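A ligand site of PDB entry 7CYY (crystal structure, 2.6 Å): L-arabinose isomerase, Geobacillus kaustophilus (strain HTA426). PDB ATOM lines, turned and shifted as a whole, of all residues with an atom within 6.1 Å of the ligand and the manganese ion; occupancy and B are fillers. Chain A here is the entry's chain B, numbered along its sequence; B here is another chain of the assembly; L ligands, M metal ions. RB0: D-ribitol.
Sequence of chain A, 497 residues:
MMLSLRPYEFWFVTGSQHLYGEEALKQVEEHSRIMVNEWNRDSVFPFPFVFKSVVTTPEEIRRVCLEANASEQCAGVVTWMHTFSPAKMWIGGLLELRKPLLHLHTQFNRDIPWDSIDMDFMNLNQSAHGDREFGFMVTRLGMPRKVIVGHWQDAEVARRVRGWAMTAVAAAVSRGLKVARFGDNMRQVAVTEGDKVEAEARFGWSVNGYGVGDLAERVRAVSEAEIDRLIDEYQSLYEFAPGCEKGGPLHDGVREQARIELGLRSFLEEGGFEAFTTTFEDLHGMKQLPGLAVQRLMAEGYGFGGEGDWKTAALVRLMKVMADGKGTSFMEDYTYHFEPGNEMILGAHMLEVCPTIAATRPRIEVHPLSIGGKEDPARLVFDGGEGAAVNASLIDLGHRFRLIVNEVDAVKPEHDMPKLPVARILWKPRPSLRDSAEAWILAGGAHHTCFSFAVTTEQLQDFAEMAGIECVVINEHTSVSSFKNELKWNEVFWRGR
A ring nitrogen (NE2) of His 129 of chain B is in hydrogen-bond range of an oxygen (O3) of the ligand (2.8 Å). OH of Tyr 20 of chain B is in hydrogen-bond range of O5 of the ligand, at 2.9 Å. NE2 of His 447 sits close to O1 of the ligand (3.0 Å). O3 of the ligand lies within hydrogen-bond range of OE1 of Gln 126 of chain B (3.4 Å).
OH of Tyr 334 touches O2 of the ligand, 3.7 Å away. Met 350 touches the ligand. Ile 371 touches the ligand. NE2 of Gln 17 of chain B touches O4 of the ligand (3.8 Å). Leu 19 of chain B touches the ligand. Phe 84 of chain B touches the ligand. 14 residues have an atom within 4 Å of the ligand: Glu 307, Glu 332, Tyr 334, His 349, Met 350, Ile 371, His 447, His 448, Gln 17 of chain B, Leu 19 of chain B, Tyr 20 of chain B, Phe 84 of chain B, Gln 126 of chain B and His 129 of chain B. The nearest printed residue that does not touch the ligand is Met 186 (4.1 Å).
The nearest printed residue that does not touch the manganese ion is His 447 (4.3 Å).
An oxygen (O1) of the ligand is bound to the manganese ion. The manganese ion is bound by OE2 of Glu 332. NE2 of His 349 is bound to the manganese ion (2.1 Å). A ring nitrogen (NE2) of His 448 is bound to the manganese ion, 2.4 Å away. The manganese ion is bound by O2 of the ligand, at 2.5 Å. The manganese ion is bound by the side-chain carboxylate (OE1) of Glu 307 (2.6 Å). The manganese ion has six donor atoms within binding distance.
The side-chain carboxylate (OE1) of Glu 332 is in hydrogen-bond range of a ring nitrogen (ND1) of His 129 of chain B, 3.1 Å away. OE1 of Glu 332 sits close to OH of Tyr 334 (3.5 Å). NE2 of His 448 lies close to NE2 of His 447 (3.3 Å). O of Glu 307 sits at hydrogen-bond distance from N of Met 186, at 3.4 Å. The side-chain hydroxyl of Tyr 20 of chain B lies close to the side-chain amide nitrogen of Gln 17 of chain B (3.3 Å). The side-chain amide oxygen of Gln 126 of chain B is in hydrogen-bond range of the backbone NH of Phe 84 of chain B, at 2.9 Å. The backbone carbonyl oxygen (O) of Phe 84 of chain B lies close to the side-chain amide nitrogen (NE2) of Gln 17 of chain B (3.5 Å). The side-chain amide nitrogen of Gln 126 of chain B lies within hydrogen-bond range of the backbone carbonyl oxygen of Met 122 of chain B.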
ATOM      1  N   MET A 186      17.149  -8.236 -29.049  1.00  0.00           N
ATOM      2  CA  MET A 186      18.330  -8.990 -29.417  1.00  0.00           C
ATOM      3  C   MET A 186      18.525  -8.911 -30.919  1.00  0.00           C
ATOM      4  O   MET A 186      17.619  -9.217 -31.693  1.00  0.00           O
ATOM      5  CB  MET A 186      18.209 -10.444 -28.966  1.00  0.00           C
ATOM      6  CG  MET A 186      19.525 -11.166 -28.968  1.00  0.00           C
ATOM      7  SD  MET A 186      19.364 -12.948 -28.853  1.00  0.00           S
ATOM      8  CE  MET A 186      20.729 -13.459 -29.884  1.00  0.00           C
ATOM      9  N   VAL A 189      17.094 -11.024 -34.241  1.00  0.00           N
ATOM     10  CA  VAL A 189      15.971 -11.891 -33.881  1.00  0.00           C
ATOM     11  C   VAL A 189      14.682 -11.365 -34.523  1.00  0.00           C
ATOM     12  O   VAL A 189      14.414 -10.158 -34.535  1.00  0.00           O
ATOM     13  CB  VAL A 189      15.804 -11.981 -32.349  1.00  0.00           C
ATOM     14  CG1 VAL A 189      14.527 -12.721 -31.988  1.00  0.00           C
ATOM     15  CG2 VAL A 189      17.036 -12.618 -31.703  1.00  0.00           C
ATOM     16  N   PHE A 280      20.396  -9.140 -22.809  1.00  0.00           N
ATOM     17  CA  PHE A 280      21.781  -9.381 -22.451  1.00  0.00           C
ATOM     18  C   PHE A 280      22.760  -8.662 -23.382  1.00  0.00           C
ATOM     19  O   PHE A 280      23.945  -8.509 -23.035  1.00  0.00           O
ATOM     20  CB  PHE A 280      22.053 -10.890 -22.434  1.00  0.00           C
ATOM     21  CG  PHE A 280      22.052 -11.524 -23.801  1.00  0.00           C
ATOM     22  CD1 PHE A 280      23.125 -11.354 -24.672  1.00  0.00           C
ATOM     23  CD2 PHE A 280      20.972 -12.310 -24.200  1.00  0.00           C
ATOM     24  CE1 PHE A 280      23.122 -11.926 -25.920  1.00  0.00           C
ATOM     25  CE2 PHE A 280      20.968 -12.891 -25.447  1.00  0.00           C
ATOM     26  CZ  PHE A 280      22.043 -12.712 -26.319  1.00  0.00           C
ATOM     27  N   GLY A 306      12.586 -12.002 -22.005  1.00  0.00           N
ATOM     28  CA  GLY A 306      13.990 -11.817 -22.292  1.00  0.00           C
ATOM     29  C   GLY A 306      14.209 -11.247 -23.679  1.00  0.00           C
ATOM     30  O   GLY A 306      13.347 -11.309 -24.548  1.00  0.00           O
ATOM     31  N   GLU A 307      15.394 -10.676 -23.869  1.00  0.00           N
ATOM     32  CA  GLU A 307      15.854 -10.229 -25.182  1.00  0.00           C
ATOM     33  C   GLU A 307      14.911  -9.190 -25.777  1.00  0.00           C
ATOM     34  O   GLU A 307      14.663  -9.172 -26.977  1.00  0.00           O
ATOM     35  CB  GLU A 307      16.037 -11.405 -26.142  1.00  0.00           C
ATOM     36  CG  GLU A 307      17.233 -12.296 -25.883  1.00  0.00           C
ATOM     37  CD  GLU A 307      16.898 -13.475 -25.001  1.00  0.00           C
ATOM     38  OE1 GLU A 307      15.721 -13.586 -24.590  1.00  0.00           O
ATOM     39  OE2 GLU A 307      17.796 -14.308 -24.717  1.00  0.00           O
ATOM     40  N   PHE A 330       7.140 -16.605 -17.503  1.00  0.00           N
ATOM     41  CA  PHE A 330       7.915 -16.556 -18.738  1.00  0.00           C
ATOM     42  C   PHE A 330       8.606 -17.901 -18.938  1.00  0.00           C
ATOM     43  O   PHE A 330       8.960 -18.573 -17.969  1.00  0.00           O
ATOM     44  CB  PHE A 330       8.944 -15.427 -18.649  1.00  0.00           C
ATOM     45  CG  PHE A 330       9.823 -15.303 -19.857  1.00  0.00           C
ATOM     46  CD1 PHE A 330       9.318 -14.824 -21.057  1.00  0.00           C
ATOM     47  CD2 PHE A 330      11.169 -15.647 -19.794  1.00  0.00           C
ATOM     48  CE1 PHE A 330      10.126 -14.701 -22.183  1.00  0.00           C
ATOM     49  CE2 PHE A 330      11.980 -15.534 -20.910  1.00  0.00           C
ATOM     50  CZ  PHE A 330      11.465 -15.062 -22.103  1.00  0.00           C
ATOM     51  N   GLU A 332      10.911 -20.587 -22.064  1.00  0.00           N
ATOM     52  CA  GLU A 332      11.516 -20.804 -23.371  1.00  0.00           C
ATOM     53  C   GLU A 332      11.835 -22.291 -23.540  1.00  0.00           C
ATOM     54  O   GLU A 332      12.355 -22.924 -22.621  1.00  0.00           O
ATOM     55  CB  GLU A 332      12.782 -19.944 -23.526  1.00  0.00           C
ATOM     56  CG  GLU A 332      13.247 -19.806 -24.942  1.00  0.00           C
ATOM     57  CD  GLU A 332      14.664 -19.277 -25.019  1.00  0.00           C
ATOM     58  OE1 GLU A 332      15.607 -20.080 -24.872  1.00  0.00           O
ATOM     59  OE2 GLU A 332      14.829 -18.058 -25.266  1.00  0.00           O
ATOM     60  N   TYR A 334      14.037 -24.946 -24.082  1.00  0.00           N
ATOM     61  CA  TYR A 334      15.487 -24.963 -24.214  1.00  0.00           C
ATOM     62  C   TYR A 334      15.988 -26.199 -24.937  1.00  0.00           C
ATOM     63  O   TYR A 334      16.859 -26.101 -25.818  1.00  0.00           O
ATOM     64  CB  TYR A 334      16.149 -24.836 -22.846  1.00  0.00           C
ATOM     65  CG  TYR A 334      16.641 -23.432 -22.677  1.00  0.00           C
ATOM     66  CD1 TYR A 334      17.896 -23.066 -23.134  1.00  0.00           C
ATOM     67  CD2 TYR A 334      15.815 -22.459 -22.153  1.00  0.00           C
ATOM     68  CE1 TYR A 334      18.341 -21.755 -23.028  1.00  0.00           C
ATOM     69  CE2 TYR A 334      16.253 -21.145 -22.042  1.00  0.00           C
ATOM     70  CZ  TYR A 334      17.534 -20.813 -22.480  1.00  0.00           C
ATOM     71  OH  TYR A 334      17.996 -19.508 -22.384  1.00  0.00           O
ATOM     72  N   HIS A 349      14.864 -20.494 -18.971  1.00  0.00           N
ATOM     73  CA  HIS A 349      15.542 -19.395 -19.644  1.00  0.00           C
ATOM     74  C   HIS A 349      16.929 -19.348 -19.044  1.00  0.00           C
ATOM     75  O   HIS A 349      17.268 -20.146 -18.170  1.00  0.00           O
ATOM     76  CB  HIS A 349      14.773 -18.069 -19.536  1.00  0.00           C
ATOM     77  CG  HIS A 349      15.065 -17.118 -20.657  1.00  0.00           C
ATOM     78  ND1 HIS A 349      15.948 -16.067 -20.544  1.00  0.00           N
ATOM     79  CD2 HIS A 349      14.609 -17.088 -21.937  1.00  0.00           C
ATOM     80  CE1 HIS A 349      16.030 -15.429 -21.700  1.00  0.00           C
ATOM     81  NE2 HIS A 349      15.225 -16.019 -22.557  1.00  0.00           N
ATOM     82  N   MET A 350      17.751 -18.402 -19.509  1.00  0.00           N
ATOM     83  CA  MET A 350      19.124 -18.370 -19.019  1.00  0.00           C
ATOM     84  C   MET A 350      19.220 -18.020 -17.551  1.00  0.00           C
ATOM     85  O   MET A 350      20.233 -18.343 -16.925  1.00  0.00           O
ATOM     86  CB  MET A 350      19.962 -17.406 -19.853  1.00  0.00           C
ATOM     87  CG  MET A 350      19.523 -15.953 -19.795  1.00  0.00           C
ATOM     88  SD  MET A 350      20.577 -14.974 -20.877  1.00  0.00           S
ATOM     89  CE  MET A 350      20.144 -15.598 -22.500  1.00  0.00           C
ATOM     90  N   ILE A 371      26.875 -15.422 -21.493  1.00  0.00           N
ATOM     91  CA  ILE A 371      26.041 -14.756 -22.496  1.00  0.00           C
ATOM     92  C   ILE A 371      26.202 -13.240 -22.401  1.00  0.00           C
ATOM     93  O   ILE A 371      26.627 -12.571 -23.363  1.00  0.00           O
ATOM     94  CB  ILE A 371      24.572 -15.187 -22.339  1.00  0.00           C
ATOM     95  CG1 ILE A 371      24.443 -16.707 -22.478  1.00  0.00           C
ATOM     96  CG2 ILE A 371      23.696 -14.541 -23.397  1.00  0.00           C
ATOM     97  CD1 ILE A 371      24.802 -17.222 -23.845  1.00  0.00           C
ATOM     98  N   HIS A 447       9.772 -18.868 -29.674  1.00  0.00           N
ATOM     99  CA  HIS A 447      10.414 -19.689 -28.662  1.00  0.00           C
ATOM    100  C   HIS A 447      10.155 -19.149 -27.267  1.00  0.00           C
ATOM    101  O   HIS A 447      10.210 -19.908 -26.280  1.00  0.00           O
ATOM    102  CB  HIS A 447      11.907 -19.746 -28.918  1.00  0.00           C
ATOM    103  CG  HIS A 447      12.574 -18.396 -28.909  1.00  0.00           C
ATOM    104  ND1 HIS A 447      12.158 -17.362 -29.716  1.00  0.00           N
ATOM    105  CD2 HIS A 447      13.615 -17.929 -28.179  1.00  0.00           C
ATOM    106  CE1 HIS A 447      12.928 -16.310 -29.492  1.00  0.00           C
ATOM    107  NE2 HIS A 447      13.805 -16.625 -28.563  1.00  0.00           N
ATOM    108  N   HIS A 448       9.892 -17.851 -27.165  1.00  0.00           N
ATOM    109  CA  HIS A 448       9.448 -17.295 -25.912  1.00  0.00           C
ATOM    110  C   HIS A 448       7.972 -17.572 -25.767  1.00  0.00           C
ATOM    111  O   HIS A 448       7.196 -17.320 -26.700  1.00  0.00           O
ATOM    112  CB  HIS A 448       9.700 -15.793 -25.840  1.00  0.00           C
ATOM    113  CG  HIS A 448      11.149 -15.445 -25.718  1.00  0.00           C
ATOM    114  ND1 HIS A 448      11.615 -14.156 -25.781  1.00  0.00           N
ATOM    115  CD2 HIS A 448      12.230 -16.233 -25.554  1.00  0.00           C
ATOM    116  CE1 HIS A 448      12.926 -14.162 -25.656  1.00  0.00           C
ATOM    117  NE2 HIS A 448      13.326 -15.407 -25.514  1.00  0.00           N
ATOM    118  N   GLN B  17      24.994 -19.163 -34.912  1.00  0.00           N
ATOM    119  CA  GLN B  17      25.401 -17.782 -34.807  1.00  0.00           C
ATOM    120  C   GLN B  17      26.825 -17.738 -34.244  1.00  0.00           C
ATOM    121  O   GLN B  17      27.416 -18.769 -33.933  1.00  0.00           O
ATOM    122  CB  GLN B  17      24.411 -16.996 -33.945  1.00  0.00           C
ATOM    123  CG  GLN B  17      24.097 -17.632 -32.578  1.00  0.00           C
ATOM    124  CD  GLN B  17      23.186 -16.721 -31.733  1.00  0.00           C
ATOM    125  OE1 GLN B  17      23.023 -15.549 -32.064  1.00  0.00           O
ATOM    126  NE2 GLN B  17      22.608 -17.264 -30.651  1.00  0.00           N
ATOM    127  N   LEU B  19      27.533 -15.981 -31.385  1.00  0.00           N
ATOM    128  CA  LEU B  19      27.442 -15.772 -29.946  1.00  0.00           C
ATOM    129  C   LEU B  19      28.229 -16.788 -29.107  1.00  0.00           C
ATOM    130  O   LEU B  19      28.983 -16.416 -28.200  1.00  0.00           O
ATOM    131  CB  LEU B  19      25.963 -15.795 -29.531  1.00  0.00           C
ATOM    132  CG  LEU B  19      25.441 -15.162 -28.229  1.00  0.00           C
ATOM    133  CD1 LEU B  19      23.920 -15.078 -28.279  1.00  0.00           C
ATOM    134  CD2 LEU B  19      25.869 -15.928 -26.984  1.00  0.00           C
ATOM    135  N   TYR B  20      28.060 -18.093 -29.381  1.00  0.00           N
ATOM    136  CA  TYR B  20      28.623 -19.116 -28.504  1.00  0.00           C
ATOM    137  C   TYR B  20      30.092 -19.396 -28.761  1.00  0.00           C
ATOM    138  O   TYR B  20      30.743 -20.031 -27.926  1.00  0.00           O
ATOM    139  CB  TYR B  20      27.810 -20.413 -28.633  1.00  0.00           C
ATOM    140  CG  TYR B  20      26.320 -20.176 -28.540  1.00  0.00           C
ATOM    141  CD1 TYR B  20      25.718 -19.952 -27.307  1.00  0.00           C
ATOM    142  CD2 TYR B  20      25.529 -20.155 -29.685  1.00  0.00           C
ATOM    143  CE1 TYR B  20      24.350 -19.731 -27.209  1.00  0.00           C
ATOM    144  CE2 TYR B  20      24.165 -19.927 -29.602  1.00  0.00           C
ATOM    145  CZ  TYR B  20      23.581 -19.715 -28.356  1.00  0.00           C
ATOM    146  OH  TYR B  20      22.230 -19.489 -28.270  1.00  0.00           O
ATOM    147  N   PHE B  84      20.291 -21.285 -31.663  1.00  0.00           N
ATOM    148  CA  PHE B  84      19.612 -20.062 -32.053  1.00  0.00           C
ATOM    149  C   PHE B  84      20.336 -19.478 -33.256  1.00  0.00           C
ATOM    150  O   PHE B  84      21.554 -19.326 -33.241  1.00  0.00           O
ATOM    151  CB  PHE B  84      19.592 -19.063 -30.884  1.00  0.00           C
ATOM    152  CG  PHE B  84      18.383 -18.157 -30.884  1.00  0.00           C
ATOM    153  CD1 PHE B  84      17.142 -18.636 -31.269  1.00  0.00           C
ATOM    154  CD2 PHE B  84      18.498 -16.840 -30.492  1.00  0.00           C
ATOM    155  CE1 PHE B  84      16.042 -17.802 -31.255  1.00  0.00           C
ATOM    156  CE2 PHE B  84      17.400 -16.010 -30.491  1.00  0.00           C
ATOM    157  CZ  PHE B  84      16.172 -16.491 -30.872  1.00  0.00           C
ATOM    158  N   MET B 119      24.814 -25.249 -18.762  1.00  0.00           N
ATOM    159  CA  MET B 119      25.131 -24.241 -19.758  1.00  0.00           C
ATOM    160  C   MET B 119      26.451 -24.627 -20.405  1.00  0.00           C
ATOM    161  O   MET B 119      27.472 -24.763 -19.706  1.00  0.00           O
ATOM    162  CB  MET B 119      25.210 -22.856 -19.129  1.00  0.00           C
ATOM    163  CG  MET B 119      23.926 -22.390 -18.448  1.00  0.00           C
ATOM    164  SD  MET B 119      22.592 -21.902 -19.562  1.00  0.00           S
ATOM    165  CE  MET B 119      23.419 -20.815 -20.725  1.00  0.00           C
ATOM    166  N   MET B 122      23.236 -26.559 -23.238  1.00  0.00           N
ATOM    167  CA  MET B 122      22.086 -25.734 -23.585  1.00  0.00           C
ATOM    168  C   MET B 122      22.487 -24.530 -24.415  1.00  0.00           C
ATOM    169  O   MET B 122      21.623 -23.889 -24.991  1.00  0.00           O
ATOM    170  CB  MET B 122      21.343 -25.319 -22.324  1.00  0.00           C
ATOM    171  CG  MET B 122      20.774 -26.532 -21.636  1.00  0.00           C
ATOM    172  SD  MET B 122      19.106 -26.260 -21.070  1.00  0.00           S
ATOM    173  CE  MET B 122      19.308 -24.619 -20.361  1.00  0.00           C
ATOM    174  N   ASN B 123      23.780 -24.208 -24.465  1.00  0.00           N
ATOM    175  CA  ASN B 123      24.274 -23.256 -25.445  1.00  0.00           C
ATOM    176  C   ASN B 123      24.303 -23.850 -26.844  1.00  0.00           C
ATOM    177  O   ASN B 123      24.183 -23.117 -27.824  1.00  0.00           O
ATOM    178  CB  ASN B 123      25.688 -22.799 -25.088  1.00  0.00           C
ATOM    179  CG  ASN B 123      25.708 -21.707 -24.055  1.00  0.00           C
ATOM    180  OD1 ASN B 123      24.668 -21.166 -23.666  1.00  0.00           O
ATOM    181  ND2 ASN B 123      26.914 -21.345 -23.609  1.00  0.00           N
ATOM    182  N   GLN B 126      20.238 -26.318 -28.907  1.00  0.00           N
ATOM    183  CA  GLN B 126      19.148 -25.382 -28.699  1.00  0.00           C
ATOM    184  C   GLN B 126      18.089 -25.475 -29.762  1.00  0.00           C
ATOM    185  O   GLN B 126      17.254 -24.572 -29.851  1.00  0.00           O
ATOM    186  CB  GLN B 126      19.673 -23.955 -28.721  1.00  0.00           C
ATOM    187  CG  GLN B 126      20.406 -23.530 -27.526  1.00  0.00           C
ATOM    188  CD  GLN B 126      21.066 -22.210 -27.763  1.00  0.00           C
ATOM    189  OE1 GLN B 126      20.931 -21.604 -28.837  1.00  0.00           O
ATOM    190  NE2 GLN B 126      21.796 -21.724 -26.759  1.00  0.00           N
ATOM    191  N   HIS B 129      14.527 -24.158 -29.375  1.00  0.00           N
ATOM    192  CA  HIS B 129      14.110 -22.788 -29.664  1.00  0.00           C
ATOM    193  C   HIS B 129      14.721 -22.222 -30.936  1.00  0.00           C
ATOM    194  O   HIS B 129      14.092 -21.395 -31.586  1.00  0.00           O
ATOM    195  CB  HIS B 129      14.399 -21.853 -28.480  1.00  0.00           C
ATOM    196  CG  HIS B 129      15.795 -21.893 -27.956  1.00  0.00           C
ATOM    197  ND1 HIS B 129      16.120 -22.521 -26.767  1.00  0.00           N
ATOM    198  CD2 HIS B 129      16.930 -21.288 -28.376  1.00  0.00           C
ATOM    199  CE1 HIS B 129      17.404 -22.343 -26.509  1.00  0.00           C
ATOM    200  NE2 HIS B 129      17.918 -21.590 -27.472  1.00  0.00           N
HETATM  201  C1  RB0 L   1      16.756 -16.622 -27.310  1.00  0.00           C
HETATM  202  O1  RB0 L   1      15.817 -16.026 -26.464  1.00  0.00           O
HETATM  203  C2  RB0 L   1      17.593 -17.565 -26.470  1.00  0.00           C
HETATM  204  O2  RB0 L   1      17.697 -17.029 -25.179  1.00  0.00           O
HETATM  205  C3  RB0 L   1      18.966 -17.764 -27.108  1.00  0.00           C
HETATM  206  O3  RB0 L   1      19.264 -19.134 -27.159  1.00  0.00           O
HETATM  207  C4  RB0 L   1      20.067 -16.994 -26.341  1.00  0.00           C
HETATM  208  O4  RB0 L   1      21.033 -16.551 -27.268  1.00  0.00           O
HETATM  209  C5  RB0 L   1      20.692 -17.867 -25.234  1.00  0.00           C
HETATM  210  O5  RB0 L   1      21.923 -18.448 -25.614  1.00  0.00           O
HETATM  211 MN    MN M   1      15.403 -16.169 -24.639  1.00  0.00          MN
